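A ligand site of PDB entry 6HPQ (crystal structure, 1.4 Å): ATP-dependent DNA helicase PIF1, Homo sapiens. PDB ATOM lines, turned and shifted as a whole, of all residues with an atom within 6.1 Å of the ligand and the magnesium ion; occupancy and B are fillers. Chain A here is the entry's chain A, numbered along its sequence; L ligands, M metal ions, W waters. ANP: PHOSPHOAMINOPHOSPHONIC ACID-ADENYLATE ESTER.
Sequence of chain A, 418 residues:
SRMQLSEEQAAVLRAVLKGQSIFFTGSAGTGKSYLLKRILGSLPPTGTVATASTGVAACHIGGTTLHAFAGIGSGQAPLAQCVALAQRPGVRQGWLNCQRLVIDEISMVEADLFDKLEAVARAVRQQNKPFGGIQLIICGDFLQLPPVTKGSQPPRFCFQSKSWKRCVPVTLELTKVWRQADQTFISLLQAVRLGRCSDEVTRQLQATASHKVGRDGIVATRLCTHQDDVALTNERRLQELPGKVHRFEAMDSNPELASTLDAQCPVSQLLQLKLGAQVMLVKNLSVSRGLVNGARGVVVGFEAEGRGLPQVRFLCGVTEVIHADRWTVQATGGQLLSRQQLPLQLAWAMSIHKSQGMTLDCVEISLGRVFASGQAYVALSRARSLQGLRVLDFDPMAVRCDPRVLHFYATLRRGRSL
N of Ser 33 is in hydrogen-bond range of O2A of the ligand. OE1 of Gln 144 sits close to O3G of the ligand (2.9 Å). The guanidinium group of Arg 179 is in salt-bridge range of an oxygen (O2G) of the ligand, at 3.0 Å. An oxygen (O3A) of the ligand sits at hydrogen-bond distance from the backbone NH (N) of Gly 31 (3.0 Å). The guanidinium group of Arg 382 is in salt-bridge range of an oxygen (O2G) of the ligand, 2.8 Å away. The side-chain amide oxygen (OE1) of Gln 9 lies within hydrogen-bond range of a nitrogen (N6) of the ligand (2.9 Å). N of Tyr 34 is in hydrogen-bond range of O2A of the ligand, 2.7 Å away. O2B of the ligand sits at hydrogen-bond distance from N of Thr 30, at 3.3 Å. O of Gln 4 is in hydrogen-bond range of N6 of the ligand (3.1 Å). The side-chain amino group (NZ) of Lys 32 is in salt-bridge range of an oxygen (O2B) of the ligand. An oxygen (O2B) of the ligand lies within hydrogen-bond range of the backbone NH (N) of Lys 32 (3.0 Å).
The side-chain hydroxyl of Ser 381 is in hydrogen-bond range of the guanidinium group of Arg 382 (2.9 Å). NH1 of Arg 382 lies close to NE2 of Gln 144 (3.4 Å). NH2 of Arg 382 sits at hydrogen-bond distance from O of Met 358 (3.2 Å). The backbone carbonyl oxygen (O) of Ser 381 lies within hydrogen-bond range of the guanidinium group (NH1) of Arg 179 (3.1 Å). O of Gly 26 lies within hydrogen-bond range of NZ of Lys 32 (3.0 Å). The backbone NH of Arg 179 sits at hydrogen-bond distance from the backbone carbonyl oxygen of Gly 29 (3.2 Å). The side-chain amide nitrogen (NE2) of Gln 356 lies close to the side-chain carboxylate (OE1) of Glu 105, at 3.5 Å. The backbone NH (N) of Ser 6 lies within hydrogen-bond range of the side-chain amide oxygen (OE1) of Gln 9 (3.0 Å).
The side-chain sulfur (SD) of Met 3 lies close to a nitrogen (N3) of the ligand, at 3.7 Å. N3B of the ligand lies close to N of Gly 29. Merely in contact with the ligand: Trp 178, Ala 28, Gly 357, Glu 105, Ser 27, Ser 6 and Leu 5. Hydrophobic or aromatic side chains within 4 Å of the ligand: Met 3, Ala 28, Tyr 34 and Trp 178.
Merely in contact with the magnesium ion: Glu 105. Two residues have an atom within 4 Å of the magnesium ion: Ser 33 and Glu 105.
The magnesium ion is bound by O1G of the ligand. Water W3 is bound to the magnesium ion (2.1 Å). O1B of the ligand binds the magnesium ion (2.1 Å). The magnesium ion is bound by water W5, 2.1 Å away. Water W7 binds the magnesium ion, 2.2 Å away. The magnesium ion is bound by OG of Ser 33 (2.2 Å). The magnesium ion has six donor atoms within binding distance.
Water W7 lies within hydrogen-bond range of the backbone carbonyl oxygen of Gly 357 (2.7 Å) and an oxygen (O1A) of the ligand (2.8 Å). Water W4 lies within hydrogen-bond range of an oxygen (O1A) of the ligand (2.7 Å), the side-chain hydroxyl of Thr 359 (2.9 Å), the guanidinium group of Arg 179 (2.9 Å) and the backbone carbonyl oxygen of Gly 357 (3.2 Å). Water W6 bridges O3' of the ligand (2.8 Å) and OG1 of Thr 359 (2.8 Å). Water W2 lies within hydrogen-bond range of an oxygen (O3G) of the ligand (2.9 Å) and the side-chain carboxylate of Glu 105 (3.2 Å). Water W11 lies within hydrogen-bond range of an oxygen (O2A) of the ligand (2.9 Å), the side-chain amino group of Lys 37 (3.2 Å) and the backbone NH of Tyr 34 (3.4 Å). Water W8 lies within hydrogen-bond range of O3' of the ligand and O of Trp 178.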
ATOM      1  N   MET A   3      15.481   7.552 -30.975  1.00  0.00           N
ATOM      2  CA  MET A   3      15.084   7.639 -29.509  1.00  0.00           C
ATOM      3  C   MET A   3      13.862   8.547 -29.347  1.00  0.00           C
ATOM      4  O   MET A   3      13.660   9.496 -30.130  1.00  0.00           O
ATOM      5  CB  MET A   3      16.216   8.181 -28.619  1.00  0.00           C
ATOM      6  CG  MET A   3      16.712   7.195 -27.574  1.00  0.00           C
ATOM      7  SD  MET A   3      18.434   7.547 -27.084  1.00  0.00           S
ATOM      8  CE  MET A   3      19.261   6.983 -28.574  1.00  0.00           C
ATOM      9  N   GLN A   4      13.082   8.263 -28.312  1.00  0.00           N
ATOM     10  CA  GLN A   4      11.902   9.072 -27.895  1.00  0.00           C
ATOM     11  C   GLN A   4      12.378  10.408 -27.304  1.00  0.00           C
ATOM     12  O   GLN A   4      12.926  10.370 -26.206  1.00  0.00           O
ATOM     13  CB  GLN A   4      11.159   8.272 -26.833  1.00  0.00           C
ATOM     14  CG  GLN A   4      10.108   9.060 -26.078  1.00  0.00           C
ATOM     15  CD  GLN A   4       8.832   9.115 -26.868  1.00  0.00           C
ATOM     16  OE1 GLN A   4       8.746   9.777 -27.902  1.00  0.00           O
ATOM     17  NE2 GLN A   4       7.834   8.384 -26.406  1.00  0.00           N
ATOM     18  N   LEU A   5      12.143  11.545 -27.949  1.00  0.00           N
ATOM     19  CA  LEU A   5      12.449  12.855 -27.320  1.00  0.00           C
ATOM     20  C   LEU A   5      11.620  13.010 -26.062  1.00  0.00           C
ATOM     21  O   LEU A   5      10.473  12.561 -26.032  1.00  0.00           O
ATOM     22  CB  LEU A   5      12.136  14.018 -28.251  1.00  0.00           C
ATOM     23  CG  LEU A   5      12.922  14.119 -29.568  1.00  0.00           C
ATOM     24  CD1 LEU A   5      12.483  15.374 -30.323  1.00  0.00           C
ATOM     25  CD2 LEU A   5      14.418  14.187 -29.312  1.00  0.00           C
ATOM     26  N   SER A   6      12.195  13.621 -25.034  1.00  0.00           N
ATOM     27  CA  SER A   6      11.439  14.005 -23.835  1.00  0.00           C
ATOM     28  C   SER A   6      10.436  15.081 -24.216  1.00  0.00           C
ATOM     29  O   SER A   6      10.557  15.727 -25.220  1.00  0.00           O
ATOM     30  CB  SER A   6      12.379  14.462 -22.789  1.00  0.00           C
ATOM     31  OG  SER A   6      13.015  15.687 -23.162  1.00  0.00           O
ATOM     32  N   GLN A   9      12.459  18.225 -24.781  1.00  0.00           N
ATOM     33  CA  GLN A   9      13.133  18.239 -26.104  1.00  0.00           C
ATOM     34  C   GLN A   9      12.096  18.510 -27.199  1.00  0.00           C
ATOM     35  O   GLN A   9      12.409  19.240 -28.137  1.00  0.00           O
ATOM     36  CB  GLN A   9      13.859  16.909 -26.302  1.00  0.00           C
ATOM     37  CG  GLN A   9      15.101  16.763 -25.416  1.00  0.00           C
ATOM     38  CD  GLN A   9      15.726  15.405 -25.591  1.00  0.00           C
ATOM     39  OE1 GLN A   9      14.999  14.415 -25.691  1.00  0.00           O
ATOM     40  NE2 GLN A   9      17.062  15.364 -25.642  1.00  0.00           N
ATOM     41  N   GLY A  26      20.647  23.885 -20.546  1.00  0.00           N
ATOM     42  CA  GLY A  26      20.553  22.728 -19.648  1.00  0.00           C
ATOM     43  C   GLY A  26      21.909  22.280 -19.197  1.00  0.00           C
ATOM     44  O   GLY A  26      22.915  22.536 -19.918  1.00  0.00           O
ATOM     45  N   SER A  27      21.934  21.522 -18.121  1.00  0.00           N
ATOM     46  CA  SER A  27      23.151  20.918 -17.553  1.00  0.00           C
ATOM     47  C   SER A  27      23.871  20.054 -18.584  1.00  0.00           C
ATOM     48  O   SER A  27      23.317  19.656 -19.631  1.00  0.00           O
ATOM     49  CB  SER A  27      22.754  20.101 -16.327  1.00  0.00           C
ATOM     50  OG  SER A  27      22.246  20.962 -15.330  1.00  0.00           O
ATOM     51  N   ALA A  28      25.125  19.753 -18.305  1.00  0.00           N
ATOM     52  CA  ALA A  28      25.892  18.766 -19.074  1.00  0.00           C
ATOM     53  C   ALA A  28      25.074  17.489 -19.191  1.00  0.00           C
ATOM     54  O   ALA A  28      24.474  16.972 -18.233  1.00  0.00           O
ATOM     55  CB  ALA A  28      27.203  18.499 -18.374  1.00  0.00           C
ATOM     56  N   GLY A  29      24.995  16.968 -20.407  1.00  0.00           N
ATOM     57  CA  GLY A  29      24.455  15.611 -20.599  1.00  0.00           C
ATOM     58  C   GLY A  29      22.930  15.553 -20.658  1.00  0.00           C
ATOM     59  O   GLY A  29      22.398  14.435 -20.563  1.00  0.00           O
ATOM     60  N   THR A  30      22.266  16.694 -20.889  1.00  0.00           N
ATOM     61  CA  THR A  30      20.800  16.789 -20.980  1.00  0.00           C
ATOM     62  C   THR A  30      20.295  16.603 -22.406  1.00  0.00           C
ATOM     63  O   THR A  30      19.103  16.644 -22.637  1.00  0.00           O
ATOM     64  CB  THR A  30      20.296  18.099 -20.366  1.00  0.00           C
ATOM     65  OG1 THR A  30      20.995  19.219 -20.969  1.00  0.00           O
ATOM     66  CG2 THR A  30      20.413  18.138 -18.857  1.00  0.00           C
ATOM     67  N   GLY A  31      21.197  16.327 -23.331  1.00  0.00           N
ATOM     68  CA  GLY A  31      20.831  16.055 -24.709  1.00  0.00           C
ATOM     69  C   GLY A  31      20.679  17.275 -25.584  1.00  0.00           C
ATOM     70  O   GLY A  31      19.906  17.217 -26.549  1.00  0.00           O
ATOM     71  N   LYS A  32      21.357  18.365 -25.297  1.00  0.00           N
ATOM     72  CA  LYS A  32      21.271  19.581 -26.146  1.00  0.00           C
ATOM     73  C   LYS A  32      21.819  19.307 -27.560  1.00  0.00           C
ATOM     74  O   LYS A  32      21.140  19.631 -28.556  1.00  0.00           O
ATOM     75  CB  LYS A  32      22.045  20.728 -25.475  1.00  0.00           C
ATOM     76  CG  LYS A  32      21.538  21.105 -24.107  1.00  0.00           C
ATOM     77  CD  LYS A  32      22.270  22.302 -23.513  1.00  0.00           C
ATOM     78  CE  LYS A  32      23.718  22.044 -23.177  1.00  0.00           C
ATOM     79  NZ  LYS A  32      23.915  20.946 -22.222  1.00  0.00           N
ATOM     80  N   SER A  33      23.005  18.751 -27.646  1.00  0.00           N
ATOM     81  CA  SER A  33      23.666  18.513 -28.971  1.00  0.00           C
ATOM     82  C   SER A  33      22.907  17.420 -29.732  1.00  0.00           C
ATOM     83  O   SER A  33      22.698  17.568 -30.953  1.00  0.00           O
ATOM     84  CB  SER A  33      25.124  18.167 -28.740  1.00  0.00           C
ATOM     85  OG  SER A  33      25.799  19.255 -28.148  1.00  0.00           O
ATOM     86  N   TYR A  34      22.463  16.401 -29.027  1.00  0.00           N
ATOM     87  CA  TYR A  34      21.579  15.355 -29.601  1.00  0.00           C
ATOM     88  C   TYR A  34      20.338  16.001 -30.202  1.00  0.00           C
ATOM     89  O   TYR A  34      19.965  15.727 -31.345  1.00  0.00           O
ATOM     90  CB  TYR A  34      21.181  14.353 -28.536  1.00  0.00           C
ATOM     91  CG  TYR A  34      20.201  13.351 -29.045  1.00  0.00           C
ATOM     92  CD1 TYR A  34      20.609  12.336 -29.891  1.00  0.00           C
ATOM     93  CD2 TYR A  34      18.857  13.458 -28.745  1.00  0.00           C
ATOM     94  CE1 TYR A  34      19.688  11.474 -30.452  1.00  0.00           C
ATOM     95  CE2 TYR A  34      17.934  12.565 -29.253  1.00  0.00           C
ATOM     96  CZ  TYR A  34      18.353  11.591 -30.126  1.00  0.00           C
ATOM     97  OH  TYR A  34      17.487  10.678 -30.671  1.00  0.00           O
ATOM     98  N   LEU A  35      19.729  16.908 -29.450  1.00  0.00           N
ATOM     99  CA  LEU A  35      18.517  17.562 -29.944  1.00  0.00           C
ATOM    100  C   LEU A  35      18.859  18.415 -31.172  1.00  0.00           C
ATOM    101  O   LEU A  35      18.052  18.492 -32.097  1.00  0.00           O
ATOM    102  CB  LEU A  35      17.881  18.358 -28.813  1.00  0.00           C
ATOM    103  CG  LEU A  35      16.605  19.118 -29.189  1.00  0.00           C
ATOM    104  CD1 LEU A  35      15.551  18.236 -29.807  1.00  0.00           C
ATOM    105  CD2 LEU A  35      16.087  19.803 -27.961  1.00  0.00           C
ATOM    106  N   LYS A  37      21.037  17.696 -33.449  1.00  0.00           N
ATOM    107  CA  LYS A  37      21.073  16.742 -34.578  1.00  0.00           C
ATOM    108  C   LYS A  37      19.632  16.444 -35.053  1.00  0.00           C
ATOM    109  O   LYS A  37      19.368  16.382 -36.277  1.00  0.00           O
ATOM    110  CB  LYS A  37      21.801  15.475 -34.169  1.00  0.00           C
ATOM    111  CG  LYS A  37      23.273  15.724 -33.958  1.00  0.00           C
ATOM    112  CD  LYS A  37      24.080  14.457 -33.729  1.00  0.00           C
ATOM    113  CE  LYS A  37      24.559  14.279 -32.320  1.00  0.00           C
ATOM    114  NZ  LYS A  37      23.841  13.167 -31.650  1.00  0.00           N
ATOM    115  N   HIS A  60      30.742  17.448 -33.406  1.00  0.00           N
ATOM    116  CA  HIS A  60      29.747  16.577 -32.747  1.00  0.00           C
ATOM    117  C   HIS A  60      28.462  16.636 -33.560  1.00  0.00           C
ATOM    118  O   HIS A  60      27.740  15.637 -33.538  1.00  0.00           O
ATOM    119  CB  HIS A  60      29.454  16.987 -31.300  1.00  0.00           C
ATOM    120  CG  HIS A  60      30.648  16.895 -30.442  1.00  0.00           C
ATOM    121  ND1 HIS A  60      30.830  17.679 -29.309  1.00  0.00           N
ATOM    122  CD2 HIS A  60      31.730  16.090 -30.554  1.00  0.00           C
ATOM    123  CE1 HIS A  60      31.983  17.335 -28.746  1.00  0.00           C
ATOM    124  NE2 HIS A  60      32.576  16.350 -29.541  1.00  0.00           N
ATOM    125  N   ASP A 104      25.790  25.664 -31.446  1.00  0.00           N
ATOM    126  CA  ASP A 104      26.034  24.906 -30.192  1.00  0.00           C
ATOM    127  C   ASP A 104      27.181  25.516 -29.390  1.00  0.00           C
ATOM    128  O   ASP A 104      28.031  26.309 -29.928  1.00  0.00           O
ATOM    129  CB  ASP A 104      26.350  23.434 -30.516  1.00  0.00           C
ATOM    130  CG  ASP A 104      26.056  22.432 -29.408  1.00  0.00           C
ATOM    131  OD1 ASP A 104      25.716  22.842 -28.223  1.00  0.00           O
ATOM    132  OD2 ASP A 104      26.153  21.209 -29.703  1.00  0.00           O
ATOM    133  N   GLU A 105      27.235  25.151 -28.109  1.00  0.00           N
ATOM    134  CA  GLU A 105      28.300  25.634 -27.181  1.00  0.00           C
ATOM    135  C   GLU A 105      28.380  27.165 -27.228  1.00  0.00           C
ATOM    136  O   GLU A 105      29.494  27.688 -27.419  1.00  0.00           O
ATOM    137  CB  GLU A 105      29.644  25.013 -27.546  1.00  0.00           C
ATOM    138  CG  GLU A 105      29.712  23.524 -27.256  1.00  0.00           C
ATOM    139  CD  GLU A 105      29.458  23.142 -25.811  1.00  0.00           C
ATOM    140  OE1 GLU A 105      29.182  24.052 -25.003  1.00  0.00           O
ATOM    141  OE2 GLU A 105      29.535  21.936 -25.490  1.00  0.00           O
ATOM    142  N   ASP A 141      25.425  25.891 -22.248  1.00  0.00           N
ATOM    143  CA  ASP A 141      25.285  25.989 -20.774  1.00  0.00           C
ATOM    144  C   ASP A 141      26.253  27.061 -20.327  1.00  0.00           C
ATOM    145  O   ASP A 141      27.459  26.826 -20.393  1.00  0.00           O
ATOM    146  CB  ASP A 141      25.616  24.652 -20.125  1.00  0.00           C
ATOM    147  CG  ASP A 141      25.460  24.636 -18.625  1.00  0.00           C
ATOM    148  OD1 ASP A 141      25.133  25.713 -18.048  1.00  0.00           O
ATOM    149  OD2 ASP A 141      25.638  23.558 -18.031  1.00  0.00           O
ATOM    150  N   GLN A 144      29.061  26.117 -18.067  1.00  0.00           N
ATOM    151  CA  GLN A 144      30.195  25.330 -18.596  1.00  0.00           C
ATOM    152  C   GLN A 144      31.305  26.275 -19.069  1.00  0.00           C
ATOM    153  O   GLN A 144      31.640  27.192 -18.306  1.00  0.00           O
ATOM    154  CB  GLN A 144      29.683  24.294 -19.586  1.00  0.00           C
ATOM    155  CG  GLN A 144      28.859  23.170 -18.937  1.00  0.00           C
ATOM    156  CD  GLN A 144      28.433  22.099 -19.920  1.00  0.00           C
ATOM    157  OE1 GLN A 144      27.265  21.686 -20.000  1.00  0.00           O
ATOM    158  NE2 GLN A 144      29.405  21.540 -20.568  1.00  0.00           N
ATOM    159  N   LEU A 174      16.331  22.101 -20.813  1.00  0.00           N
ATOM    160  CA  LEU A 174      16.364  20.616 -20.768  1.00  0.00           C
ATOM    161  C   LEU A 174      16.919  20.325 -19.366  1.00  0.00           C
ATOM    162  O   LEU A 174      17.988  20.797 -19.082  1.00  0.00           O
ATOM    163  CB  LEU A 174      17.301  20.069 -21.847  1.00  0.00           C
ATOM    164  CG  LEU A 174      16.963  20.431 -23.298  1.00  0.00           C
ATOM    165  CD1 LEU A 174      17.879  19.657 -24.250  1.00  0.00           C
ATOM    166  CD2 LEU A 174      15.505  20.173 -23.647  1.00  0.00           C
ATOM    167  N   TRP A 178      20.930  12.619 -19.064  1.00  0.00           N
ATOM    168  CA  TRP A 178      21.002  11.267 -19.660  1.00  0.00           C
ATOM    169  C   TRP A 178      22.426  10.702 -19.635  1.00  0.00           C
ATOM    170  O   TRP A 178      22.568   9.492 -19.624  1.00  0.00           O
ATOM    171  CB  TRP A 178      20.467  11.267 -21.084  1.00  0.00           C
ATOM    172  CG  TRP A 178      19.124  11.897 -21.283  1.00  0.00           C
ATOM    173  CD1 TRP A 178      18.802  13.146 -21.773  1.00  0.00           C
ATOM    174  CD2 TRP A 178      17.892  11.229 -21.097  1.00  0.00           C
ATOM    175  NE1 TRP A 178      17.443  13.306 -21.815  1.00  0.00           N
ATOM    176  CE2 TRP A 178      16.859  12.132 -21.439  1.00  0.00           C
ATOM    177  CE3 TRP A 178      17.597   9.964 -20.629  1.00  0.00           C
ATOM    178  CZ2 TRP A 178      15.517  11.765 -21.331  1.00  0.00           C
ATOM    179  CZ3 TRP A 178      16.269   9.605 -20.561  1.00  0.00           C
ATOM    180  CH2 TRP A 178      15.253  10.492 -20.896  1.00  0.00           C
ATOM    181  N   ARG A 179      23.441  11.549 -19.694  1.00  0.00           N
ATOM    182  CA  ARG A 179      24.836  11.038 -19.839  1.00  0.00           C
ATOM    183  C   ARG A 179      25.163  10.110 -18.669  1.00  0.00           C
ATOM    184  O   ARG A 179      25.689   9.008 -18.907  1.00  0.00           O
ATOM    185  CB  ARG A 179      25.889  12.149 -19.878  1.00  0.00           C
ATOM    186  CG  ARG A 179      27.328  11.652 -19.940  1.00  0.00           C
ATOM    187  CD  ARG A 179      28.326  12.801 -19.998  1.00  0.00           C
ATOM    188  NE  ARG A 179      28.250  13.442 -21.330  1.00  0.00           N
ATOM    189  CZ  ARG A 179      28.295  14.740 -21.586  1.00  0.00           C
ATOM    190  NH1 ARG A 179      28.411  15.636 -20.593  1.00  0.00           N
ATOM    191  NH2 ARG A 179      28.188  15.150 -22.850  1.00  0.00           N
ATOM    192  N   GLN A 356      35.258  19.104 -24.572  1.00  0.00           N
ATOM    193  CA  GLN A 356      33.976  19.836 -24.624  1.00  0.00           C
ATOM    194  C   GLN A 356      32.925  19.050 -25.400  1.00  0.00           C
ATOM    195  O   GLN A 356      33.181  18.592 -26.495  1.00  0.00           O
ATOM    196  CB  GLN A 356      34.176  21.225 -25.258  1.00  0.00           C
ATOM    197  CG  GLN A 356      32.904  22.017 -25.393  1.00  0.00           C
ATOM    198  CD  GLN A 356      33.153  23.331 -26.079  1.00  0.00           C
ATOM    199  OE1 GLN A 356      33.843  23.367 -27.105  1.00  0.00           O
ATOM    200  NE2 GLN A 356      32.621  24.420 -25.513  1.00  0.00           N
ATOM    201  N   GLY A 357      31.796  18.832 -24.778  1.00  0.00           N
ATOM    202  CA  GLY A 357      30.662  18.167 -25.403  1.00  0.00           C
ATOM    203  C   GLY A 357      30.760  16.643 -25.486  1.00  0.00           C
ATOM    204  O   GLY A 357      29.740  16.050 -25.884  1.00  0.00           O
ATOM    205  N   MET A 358      31.843  16.042 -25.022  1.00  0.00           N
ATOM    206  CA  MET A 358      32.095  14.580 -25.112  1.00  0.00           C
ATOM    207  C   MET A 358      31.585  13.839 -23.885  1.00  0.00           C
ATOM    208  O   MET A 358      31.513  14.421 -22.814  1.00  0.00           O
ATOM    209  CB  MET A 358      33.602  14.293 -25.249  1.00  0.00           C
ATOM    210  CG  MET A 358      34.167  14.853 -26.538  1.00  0.00           C
ATOM    211  SD  MET A 358      35.819  14.304 -26.832  1.00  0.00           S
ATOM    212  CE  MET A 358      35.650  12.561 -27.222  1.00  0.00           C
ATOM    213  N   THR A 359      31.373  12.536 -24.022  1.00  0.00           N
ATOM    214  CA  THR A 359      31.260  11.578 -22.932  1.00  0.00           C
ATOM    215  C   THR A 359      32.561  10.789 -22.880  1.00  0.00           C
ATOM    216  O   THR A 359      32.969  10.249 -23.910  1.00  0.00           O
ATOM    217  CB  THR A 359      30.023  10.693 -23.147  1.00  0.00           C
ATOM    218  OG1 THR A 359      28.821  11.479 -23.281  1.00  0.00           O
ATOM    219  CG2 THR A 359      29.905   9.698 -22.016  1.00  0.00           C
ATOM    220  N   SER A 381      31.837  16.363 -15.381  1.00  0.00           N
ATOM    221  CA  SER A 381      30.586  15.992 -16.055  1.00  0.00           C
ATOM    222  C   SER A 381      30.849  15.261 -17.375  1.00  0.00           C
ATOM    223  O   SER A 381      29.861  14.889 -18.014  1.00  0.00           O
ATOM    224  CB  SER A 381      29.681  17.200 -16.249  1.00  0.00           C
ATOM    225  OG  SER A 381      30.252  18.186 -17.067  1.00  0.00           O
ATOM    226  N   ARG A 382      32.098  15.075 -17.762  1.00  0.00           N
ATOM    227  CA  ARG A 382      32.398  14.223 -18.937  1.00  0.00           C
ATOM    228  C   ARG A 382      32.135  12.756 -18.610  1.00  0.00           C
ATOM    229  O   ARG A 382      31.785  12.019 -19.526  1.00  0.00           O
ATOM    230  CB  ARG A 382      33.852  14.364 -19.388  1.00  0.00           C
ATOM    231  CG  ARG A 382      34.271  15.752 -19.844  1.00  0.00           C
ATOM    232  CD  ARG A 382      33.329  16.451 -20.796  1.00  0.00           C
ATOM    233  NE  ARG A 382      32.250  17.143 -20.105  1.00  0.00           N
ATOM    234  CZ  ARG A 382      31.218  17.649 -20.701  1.00  0.00           C
ATOM    235  NH1 ARG A 382      30.358  18.372 -19.997  1.00  0.00           N
ATOM    236  NH2 ARG A 382      31.019  17.475 -22.009  1.00  0.00           N
HETATM  237  PG  ANP L   1      27.173  18.790 -22.967  1.00  0.00           P
HETATM  238  O1G ANP L   1      27.558  19.213 -24.386  1.00  0.00           O
HETATM  239  O2G ANP L   1      28.283  18.110 -22.202  1.00  0.00           O
HETATM  240  O3G ANP L   1      26.509  19.910 -22.206  1.00  0.00           O
HETATM  241  PB  ANP L   1      24.595  17.790 -24.067  1.00  0.00           P
HETATM  242  O1B ANP L   1      24.913  18.370 -25.412  1.00  0.00           O
HETATM  243  O2B ANP L   1      23.531  18.487 -23.289  1.00  0.00           O
HETATM  244  N3B ANP L   1      25.965  17.610 -23.182  1.00  0.00           N
HETATM  245  PA  ANP L   1      24.457  15.267 -25.476  1.00  0.00           P
HETATM  246  O1A ANP L   1      25.928  15.072 -25.428  1.00  0.00           O
HETATM  247  O2A ANP L   1      23.745  15.700 -26.702  1.00  0.00           O
HETATM  248  O3A ANP L   1      24.084  16.277 -24.273  1.00  0.00           O
HETATM  249  O5' ANP L   1      23.712  13.930 -24.948  1.00  0.00           O
HETATM  250  C5' ANP L   1      24.162  13.191 -23.847  1.00  0.00           C
HETATM  251  C4' ANP L   1      23.581  11.820 -23.940  1.00  0.00           C
HETATM  252  O4' ANP L   1      22.148  11.945 -23.814  1.00  0.00           O
HETATM  253  C3' ANP L   1      23.797  11.116 -25.293  1.00  0.00           C
HETATM  254  O3' ANP L   1      24.475   9.883 -25.176  1.00  0.00           O
HETATM  255  C2' ANP L   1      22.395  10.813 -25.812  1.00  0.00           C
HETATM  256  O2' ANP L   1      22.456   9.530 -26.359  1.00  0.00           O
HETATM  257  C1' ANP L   1      21.531  10.932 -24.560  1.00  0.00           C
HETATM  258  N9  ANP L   1      20.171  11.350 -24.822  1.00  0.00           N
HETATM  259  C8  ANP L   1      19.777  12.542 -25.320  1.00  0.00           C
HETATM  260  N7  ANP L   1      18.462  12.649 -25.422  1.00  0.00           N
HETATM  261  C5  ANP L   1      17.961  11.459 -24.918  1.00  0.00           C
HETATM  262  C6  ANP L   1      16.645  10.974 -24.758  1.00  0.00           C
HETATM  263  N6  ANP L   1      15.528  11.644 -25.100  1.00  0.00           N
HETATM  264  N1  ANP L   1      16.527   9.733 -24.210  1.00  0.00           N
HETATM  265  C2  ANP L   1      17.639   9.097 -23.855  1.00  0.00           C
HETATM  266  N3  ANP L   1      18.924   9.425 -23.992  1.00  0.00           N
HETATM  267  C4  ANP L   1      19.022  10.656 -24.528  1.00  0.00           C
HETATM  268 MG    MG M   1      26.690  19.214 -26.147  1.00  0.00          MG
HETATM  269  O   HOH W   1      26.905  10.673 -26.705  1.00  0.00           O
HETATM  270  O   HOH W   2      26.886  22.364 -23.660  1.00  0.00           O
HETATM  271  O   HOH W   3      25.960  21.137 -26.035  1.00  0.00           O
HETATM  272  O   HOH W   4      28.080  13.432 -25.245  1.00  0.00           O
HETATM  273  O   HOH W   5      28.452  19.887 -27.075  1.00  0.00           O
HETATM  274  O   HOH W   6      26.404  10.099 -23.197  1.00  0.00           O
HETATM  275  O   HOH W   7      27.337  17.193 -26.576  1.00  0.00           O
HETATM  276  O   HOH W   8      23.222   8.212 -22.700  1.00  0.00           O
HETATM  277  O   HOH W   9      14.394   8.190 -23.700  1.00  0.00           O
HETATM  278  O   HOH W  10      20.584   7.602 -22.780  1.00  0.00           O
HETATM  279  O   HOH W  11      24.970  14.125 -28.795  1.00  0.00           O
